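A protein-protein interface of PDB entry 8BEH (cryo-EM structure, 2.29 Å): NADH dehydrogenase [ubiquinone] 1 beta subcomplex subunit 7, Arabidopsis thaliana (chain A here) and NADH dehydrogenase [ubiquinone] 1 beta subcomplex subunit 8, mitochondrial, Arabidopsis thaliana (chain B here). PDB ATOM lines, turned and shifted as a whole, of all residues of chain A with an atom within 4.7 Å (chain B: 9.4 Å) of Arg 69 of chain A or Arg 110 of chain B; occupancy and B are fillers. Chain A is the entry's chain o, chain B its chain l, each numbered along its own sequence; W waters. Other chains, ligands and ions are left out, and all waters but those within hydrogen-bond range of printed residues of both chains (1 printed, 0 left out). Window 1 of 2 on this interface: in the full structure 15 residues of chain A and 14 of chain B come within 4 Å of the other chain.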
ATOM      1  N   GLY A  25      -0.750  -9.899 -34.844  1.00  0.00           N
ATOM      2  CA  GLY A  25      -0.332  -9.329 -33.574  1.00  0.00           C
ATOM      3  C   GLY A  25      -0.455 -10.250 -32.377  1.00  0.00           C
ATOM      4  O   GLY A  25      -0.004  -9.883 -31.371  1.00  0.00           O
ATOM      5  N   LEU A  65       5.083 -11.981 -20.279  1.00  0.00           N
ATOM      6  CA  LEU A  65       5.789 -11.315 -21.375  1.00  0.00           C
ATOM      7  C   LEU A  65       5.937  -9.819 -21.103  1.00  0.00           C
ATOM      8  O   LEU A  65       7.037  -9.245 -21.217  1.00  0.00           O
ATOM      9  CB  LEU A  65       5.048 -11.546 -22.693  1.00  0.00           C
ATOM     10  CG  LEU A  65       5.377 -12.781 -23.535  1.00  0.00           C
ATOM     11  CD1 LEU A  65       4.987 -12.564 -24.991  1.00  0.00           C
ATOM     12  CD2 LEU A  65       6.848 -13.146 -23.429  1.00  0.00           C
ATOM     13  N   VAL A  66       4.832  -9.175 -20.720  1.00  0.00           N
ATOM     14  CA  VAL A  66       4.873  -7.744 -20.432  1.00  0.00           C
ATOM     15  C   VAL A  66       5.804  -7.453 -19.263  1.00  0.00           C
ATOM     16  O   VAL A  66       6.540  -6.461 -19.272  1.00  0.00           O
ATOM     17  CB  VAL A  66       3.456  -7.199 -20.177  1.00  0.00           C
ATOM     18  CG1 VAL A  66       3.502  -5.703 -19.978  1.00  0.00           C
ATOM     19  CG2 VAL A  66       2.553  -7.529 -21.341  1.00  0.00           C
ATOM     20  N   MET A  67       5.781  -8.300 -18.236  1.00  0.00           N
ATOM     21  CA  MET A  67       6.641  -8.073 -17.077  1.00  0.00           C
ATOM     22  C   MET A  67       8.114  -8.158 -17.453  1.00  0.00           C
ATOM     23  O   MET A  67       8.926  -7.361 -16.973  1.00  0.00           O
ATOM     24  CB  MET A  67       6.307  -9.063 -15.966  1.00  0.00           C
ATOM     25  CG  MET A  67       5.002  -8.771 -15.271  1.00  0.00           C
ATOM     26  SD  MET A  67       4.853  -7.037 -14.816  1.00  0.00           S
ATOM     27  CE  MET A  67       3.389  -6.579 -15.739  1.00  0.00           C
ATOM     28  N   GLU A  68       8.482  -9.117 -18.304  1.00  0.00           N
ATOM     29  CA  GLU A  68       9.875  -9.201 -18.733  1.00  0.00           C
ATOM     30  C   GLU A  68      10.285  -7.949 -19.496  1.00  0.00           C
ATOM     31  O   GLU A  68      11.388  -7.426 -19.300  1.00  0.00           O
ATOM     32  CB  GLU A  68      10.115 -10.445 -19.589  1.00  0.00           C
ATOM     33  CG  GLU A  68       9.657 -11.737 -18.957  1.00  0.00           C
ATOM     34  CD  GLU A  68       9.605 -12.879 -19.950  1.00  0.00           C
ATOM     35  OE1 GLU A  68       8.767 -12.828 -20.874  1.00  0.00           O
ATOM     36  OE2 GLU A  68      10.405 -13.829 -19.806  1.00  0.00           O
ATOM     37  N   ARG A  69       9.486  -7.422 -20.391  1.00  0.00           N
ATOM     38  CA  ARG A  69       9.764  -6.156 -21.112  1.00  0.00           C
ATOM     39  C   ARG A  69       9.756  -4.953 -20.145  1.00  0.00           C
ATOM     40  O   ARG A  69      10.429  -3.990 -20.404  1.00  0.00           O
ATOM     41  CB  ARG A  69       8.808  -6.139 -22.320  1.00  0.00           C
ATOM     42  CG  ARG A  69       9.153  -6.999 -23.517  1.00  0.00           C
ATOM     43  CD  ARG A  69       7.986  -6.988 -24.491  1.00  0.00           C
ATOM     44  NE  ARG A  69       7.496  -5.646 -24.758  1.00  0.00           N
ATOM     45  CZ  ARG A  69       6.221  -5.302 -24.854  1.00  0.00           C
ATOM     46  NH1 ARG A  69       5.274  -6.211 -24.740  1.00  0.00           N
ATOM     47  NH2 ARG A  69       5.897  -4.046 -25.084  1.00  0.00           N
ATOM     48  N   MET A  70       9.028  -5.018 -19.047  1.00  0.00           N
ATOM     49  CA  MET A  70       9.112  -3.956 -18.046  1.00  0.00           C
ATOM     50  C   MET A  70      10.431  -4.008 -17.277  1.00  0.00           C
ATOM     51  O   MET A  70      11.055  -2.969 -17.034  1.00  0.00           O
ATOM     52  CB  MET A  70       7.925  -4.043 -17.087  1.00  0.00           C
ATOM     53  CG  MET A  70       6.586  -3.737 -17.728  1.00  0.00           C
ATOM     54  SD  MET A  70       5.228  -3.593 -16.556  1.00  0.00           S
ATOM     55  CE  MET A  70       5.561  -1.993 -15.836  1.00  0.00           C
ATOM     56  N   LEU A  71      10.873  -5.208 -16.878  1.00  0.00           N
ATOM     57  CA  LEU A  71      12.169  -5.322 -16.205  1.00  0.00           C
ATOM     58  C   LEU A  71      13.315  -4.940 -17.132  1.00  0.00           C
ATOM     59  O   LEU A  71      14.288  -4.309 -16.699  1.00  0.00           O
ATOM     60  CB  LEU A  71      12.386  -6.730 -15.646  1.00  0.00           C
ATOM     61  CG  LEU A  71      11.788  -7.041 -14.269  1.00  0.00           C
ATOM     62  CD1 LEU A  71      10.471  -7.792 -14.357  1.00  0.00           C
ATOM     63  CD2 LEU A  71      12.787  -7.810 -13.428  1.00  0.00           C
ATOM     64  N   ALA A  72      13.224  -5.313 -18.409  1.00  0.00           N
ATOM     65  CA  ALA A  72      14.247  -4.909 -19.366  1.00  0.00           C
ATOM     66  C   ALA A  72      14.340  -3.390 -19.460  1.00  0.00           C
ATOM     67  O   ALA A  72      15.439  -2.819 -19.445  1.00  0.00           O
ATOM     68  CB  ALA A  72      13.948  -5.519 -20.733  1.00  0.00           C
ATOM     69  N   MET A  73      13.191  -2.712 -19.547  1.00  0.00           N
ATOM     70  CA  MET A  73      13.225  -1.253 -19.596  1.00  0.00           C
ATOM     71  C   MET A  73      13.721  -0.660 -18.282  1.00  0.00           C
ATOM     72  O   MET A  73      14.366   0.390 -18.289  1.00  0.00           O
ATOM     73  CB  MET A  73      11.847  -0.695 -19.948  1.00  0.00           C
ATOM     74  CG  MET A  73      11.795   0.822 -20.069  1.00  0.00           C
ATOM     75  SD  MET A  73      13.061   1.520 -21.151  1.00  0.00           S
ATOM     76  CE  MET A  73      12.368   1.207 -22.769  1.00  0.00           C
ATOM     77  N   VAL B 105       8.566   5.669 -21.694  1.00  0.00           N
ATOM     78  CA  VAL B 105       7.772   4.440 -21.803  1.00  0.00           C
ATOM     79  C   VAL B 105       8.358   3.382 -20.870  1.00  0.00           C
ATOM     80  O   VAL B 105       9.588   3.205 -20.833  1.00  0.00           O
ATOM     81  CB  VAL B 105       7.730   3.954 -23.260  1.00  0.00           C
ATOM     82  CG1 VAL B 105       9.123   3.894 -23.852  1.00  0.00           C
ATOM     83  CG2 VAL B 105       7.037   2.606 -23.364  1.00  0.00           C
ATOM     84  N   PRO B 106       7.542   2.686 -20.082  1.00  0.00           N
ATOM     85  CA  PRO B 106       8.065   1.767 -19.061  1.00  0.00           C
ATOM     86  C   PRO B 106       8.313   0.340 -19.531  1.00  0.00           C
ATOM     87  O   PRO B 106       8.489  -0.536 -18.681  1.00  0.00           O
ATOM     88  CB  PRO B 106       6.945   1.794 -18.017  1.00  0.00           C
ATOM     89  CG  PRO B 106       5.723   1.896 -18.855  1.00  0.00           C
ATOM     90  CD  PRO B 106       6.087   2.868 -19.944  1.00  0.00           C
ATOM     91  N   PHE B 107       8.313   0.075 -20.835  1.00  0.00           N
ATOM     92  CA  PHE B 107       8.639  -1.241 -21.362  1.00  0.00           C
ATOM     93  C   PHE B 107       9.415  -1.081 -22.659  1.00  0.00           C
ATOM     94  O   PHE B 107       9.298  -0.067 -23.349  1.00  0.00           O
ATOM     95  CB  PHE B 107       7.386  -2.108 -21.593  1.00  0.00           C
ATOM     96  CG  PHE B 107       6.241  -1.372 -22.229  1.00  0.00           C
ATOM     97  CD1 PHE B 107       6.214  -1.144 -23.596  1.00  0.00           C
ATOM     98  CD2 PHE B 107       5.190  -0.908 -21.459  1.00  0.00           C
ATOM     99  CE1 PHE B 107       5.161  -0.468 -24.177  1.00  0.00           C
ATOM    100  CE2 PHE B 107       4.137  -0.231 -22.038  1.00  0.00           C
ATOM    101  CZ  PHE B 107       4.125  -0.012 -23.398  1.00  0.00           C
ATOM    102  N   THR B 108      10.228  -2.085 -22.897  1.00  0.00           N
ATOM    103  CA  THR B 108      10.959  -2.110 -24.171  1.00  0.00           C
ATOM    104  C   THR B 108       9.935  -2.392 -25.265  1.00  0.00           C
ATOM    105  O   THR B 108       8.888  -2.924 -24.993  1.00  0.00           O
ATOM    106  CB  THR B 108      12.125  -3.098 -24.168  1.00  0.00           C
ATOM    107  OG1 THR B 108      11.603  -4.405 -23.965  1.00  0.00           O
ATOM    108  CG2 THR B 108      13.189  -2.766 -23.151  1.00  0.00           C
ATOM    109  N   PRO B 109      10.267  -2.116 -26.523  1.00  0.00           N
ATOM    110  CA  PRO B 109       9.358  -2.474 -27.605  1.00  0.00           C
ATOM    111  C   PRO B 109       9.227  -3.997 -27.768  1.00  0.00           C
ATOM    112  O   PRO B 109      10.170  -4.694 -27.455  1.00  0.00           O
ATOM    113  CB  PRO B 109       9.994  -1.758 -28.837  1.00  0.00           C
ATOM    114  CG  PRO B 109      11.033  -0.845 -28.281  1.00  0.00           C
ATOM    115  CD  PRO B 109      11.490  -1.486 -26.995  1.00  0.00           C
ATOM    116  N   ARG B 110       8.031  -4.431 -28.198  1.00  0.00           N
ATOM    117  CA  ARG B 110       7.758  -5.874 -28.423  1.00  0.00           C
ATOM    118  C   ARG B 110       8.669  -6.397 -29.523  1.00  0.00           C
ATOM    119  O   ARG B 110       9.053  -5.610 -30.416  1.00  0.00           O
ATOM    120  CB  ARG B 110       6.341  -6.131 -28.942  1.00  0.00           C
ATOM    121  CG  ARG B 110       5.217  -5.863 -27.955  1.00  0.00           C
ATOM    122  CD  ARG B 110       3.876  -6.286 -28.516  1.00  0.00           C
ATOM    123  NE  ARG B 110       2.815  -6.245 -27.521  1.00  0.00           N
ATOM    124  CZ  ARG B 110       1.590  -6.723 -27.703  1.00  0.00           C
ATOM    125  NH1 ARG B 110       1.264  -7.299 -28.847  1.00  0.00           N
ATOM    126  NH2 ARG B 110       0.698  -6.643 -26.735  1.00  0.00           N
ATOM    127  N   VAL B 111       8.942  -7.694 -29.483  1.00  0.00           N
ATOM    128  CA  VAL B 111       9.821  -8.320 -30.496  1.00  0.00           C
ATOM    129  C   VAL B 111       9.137  -9.612 -30.802  1.00  0.00           C
ATOM    130  O   VAL B 111       9.059 -10.459 -29.946  1.00  0.00           O
ATOM    131  CB  VAL B 111      11.304  -8.454 -30.098  1.00  0.00           C
ATOM    132  CG1 VAL B 111      12.076  -9.244 -31.138  1.00  0.00           C
ATOM    133  CG2 VAL B 111      11.950  -7.110 -29.848  1.00  0.00           C
ATOM    134  N   TYR B 112       8.663  -9.683 -32.017  1.00  0.00           N
ATOM    135  CA  TYR B 112       7.955 -10.874 -32.459  1.00  0.00           C
ATOM    136  C   TYR B 112       8.987 -11.904 -32.872  1.00  0.00           C
ATOM    137  O   TYR B 112      10.032 -11.506 -33.291  1.00  0.00           O
ATOM    138  CB  TYR B 112       6.932 -10.494 -33.544  1.00  0.00           C
ATOM    139  CG  TYR B 112       5.721  -9.843 -32.947  1.00  0.00           C
ATOM    140  CD1 TYR B 112       5.710  -8.493 -32.637  1.00  0.00           C
ATOM    141  CD2 TYR B 112       4.615 -10.601 -32.627  1.00  0.00           C
ATOM    142  CE1 TYR B 112       4.593  -7.905 -32.075  1.00  0.00           C
ATOM    143  CE2 TYR B 112       3.492 -10.027 -32.073  1.00  0.00           C
ATOM    144  CZ  TYR B 112       3.482  -8.674 -31.801  1.00  0.00           C
ATOM    145  OH  TYR B 112       2.378  -8.121 -31.244  1.00  0.00           O
ATOM    146  N   PRO B 113       8.648 -13.196 -32.841  1.00  0.00           N
ATOM    147  CA  PRO B 113       9.530 -14.251 -33.352  1.00  0.00           C
ATOM    148  C   PRO B 113       9.591 -14.293 -34.871  1.00  0.00           C
ATOM    149  O   PRO B 113       8.885 -13.546 -35.560  1.00  0.00           O
ATOM    150  CB  PRO B 113       8.904 -15.531 -32.786  1.00  0.00           C
ATOM    151  CG  PRO B 113       7.458 -15.187 -32.653  1.00  0.00           C
ATOM    152  CD  PRO B 113       7.431 -13.751 -32.221  1.00  0.00           C
ATOM    153  N   ASN B 116      10.815 -10.950 -36.575  1.00  0.00           N
ATOM    154  CA  ASN B 116       9.725  -9.957 -36.451  1.00  0.00           C
ATOM    155  C   ASN B 116       8.596 -10.261 -37.470  1.00  0.00           C
ATOM    156  O   ASN B 116       8.024  -9.333 -37.893  1.00  0.00           O
ATOM    157  CB  ASN B 116      10.299  -8.543 -36.282  1.00  0.00           C
ATOM    158  CG  ASN B 116      10.102  -8.003 -34.891  1.00  0.00           C
ATOM    159  OD1 ASN B 116       8.980  -7.734 -34.478  1.00  0.00           O
ATOM    160  ND2 ASN B 116      11.191  -7.874 -34.158  1.00  0.00           N
ATOM    161  N   LEU B 117       8.242 -11.556 -37.638  1.00  0.00           N
ATOM    162  CA  LEU B 117       7.185 -11.952 -38.568  1.00  0.00           C
ATOM    163  C   LEU B 117       7.392 -11.333 -39.948  1.00  0.00           C
ATOM    164  O   LEU B 117       6.496 -10.715 -40.524  1.00  0.00           O
ATOM    165  CB  LEU B 117       5.803 -11.595 -38.015  1.00  0.00           C
ATOM    166  CG  LEU B 117       5.408 -12.135 -36.641  1.00  0.00           C
ATOM    167  CD1 LEU B 117       4.168 -11.424 -36.137  1.00  0.00           C
ATOM    168  CD2 LEU B 117       5.184 -13.635 -36.705  1.00  0.00           C
HETATM  169  O   HOH W   1       3.795  -8.300 -25.525  1.00  0.00           O
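The guanidinium group (NE) of Arg 69 of chain A lies within hydrogen-bond range of the backbone carbonyl oxygen (O) of Thr 108 of chain B, at 3.1 Å. OH of Tyr 112 of chain B sits at hydrogen-bond distance from O of Gly 25 of chain A (3.0 Å).
The backbone NH (N) of Tyr 112 of chain B lies within hydrogen-bond range of the side-chain amide oxygen (OD1) of Asn 116 of chain B (3.2 Å). OH of Tyr 112 of chain B sits at hydrogen-bond distance from NH1 of Arg 110 of chain B, at 2.8 Å.
Among the printed residues, merely in contact across the chains: Arg 69 of chain A with Arg 110 of chain B (3.2 Å), Arg 69 of chain A with Phe 107 of chain B (3.3 Å), Met 73 of chain A with Val 105 of chain B (3.3 Å), Met 73 of chain A with Phe 107 of chain B (3.4 Å), Met 70 of chain A with Pro 106 of chain B (3.5 Å), Met 73 of chain A with Pro 106 of chain B (3.6 Å), Met 73 of chain A with Thr 108 of chain B (3.6 Å), Ala 72 of chain A with Thr 108 of chain B (3.7 Å), Gly 25 of chain A with Arg 110 of chain B (3.8 Å) and Arg 69 of chain A with Pro 109 of chain B (3.8 Å).
Of chain B, only Phe 107 (3.3 Å), Thr 108 (3.1 Å), Pro 109 (3.8 Å) and Arg 110 (3.2 Å) come within 4 Å of Arg 69 of chain A. Ala 72 of chain A touches just one residue of chain B: Thr 108 (3.7 Å). Of the printed residues of chain A, Pro 109 of chain B touches Arg 69. Arg 110 of chain B touches two residues of chain A. Of the printed residues of chain A, Tyr 112 of chain B touches Gly 25. The nearest residue of chain B that does not touch Arg 69 of chain A is Pro 106 of chain B (4.3 Å). The nearest printed residue of chain A that does not touch Arg 110 of chain B is Val 66 of chain A (5.8 Å).
Of the 11 printed residues of chain B, 7 touch a printed residue of chain A. Printed residues of chain B that touch a printed residue of chain A: Val 105, Pro 106, Phe 107, Thr 108, Pro 109, Arg 110 and Tyr 112. Of the 10 printed residues of chain A, 5 touch a printed residue of chain B. Printed residues of chain A that touch a printed residue of chain B: Gly 25, Arg 69, Met 70, Ala 72 and Met 73. Hydrophobic or aromatic side chains of chain A that line the printed part of chain B: Met 70, Ala 72 and Met 73. Among the printed residues, 12 pairs touch across the chains.
Water W1 bridges NH1 of Arg 69 of chain A (2.7 Å) and NE of Arg 110 of chain B (3.0 Å).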
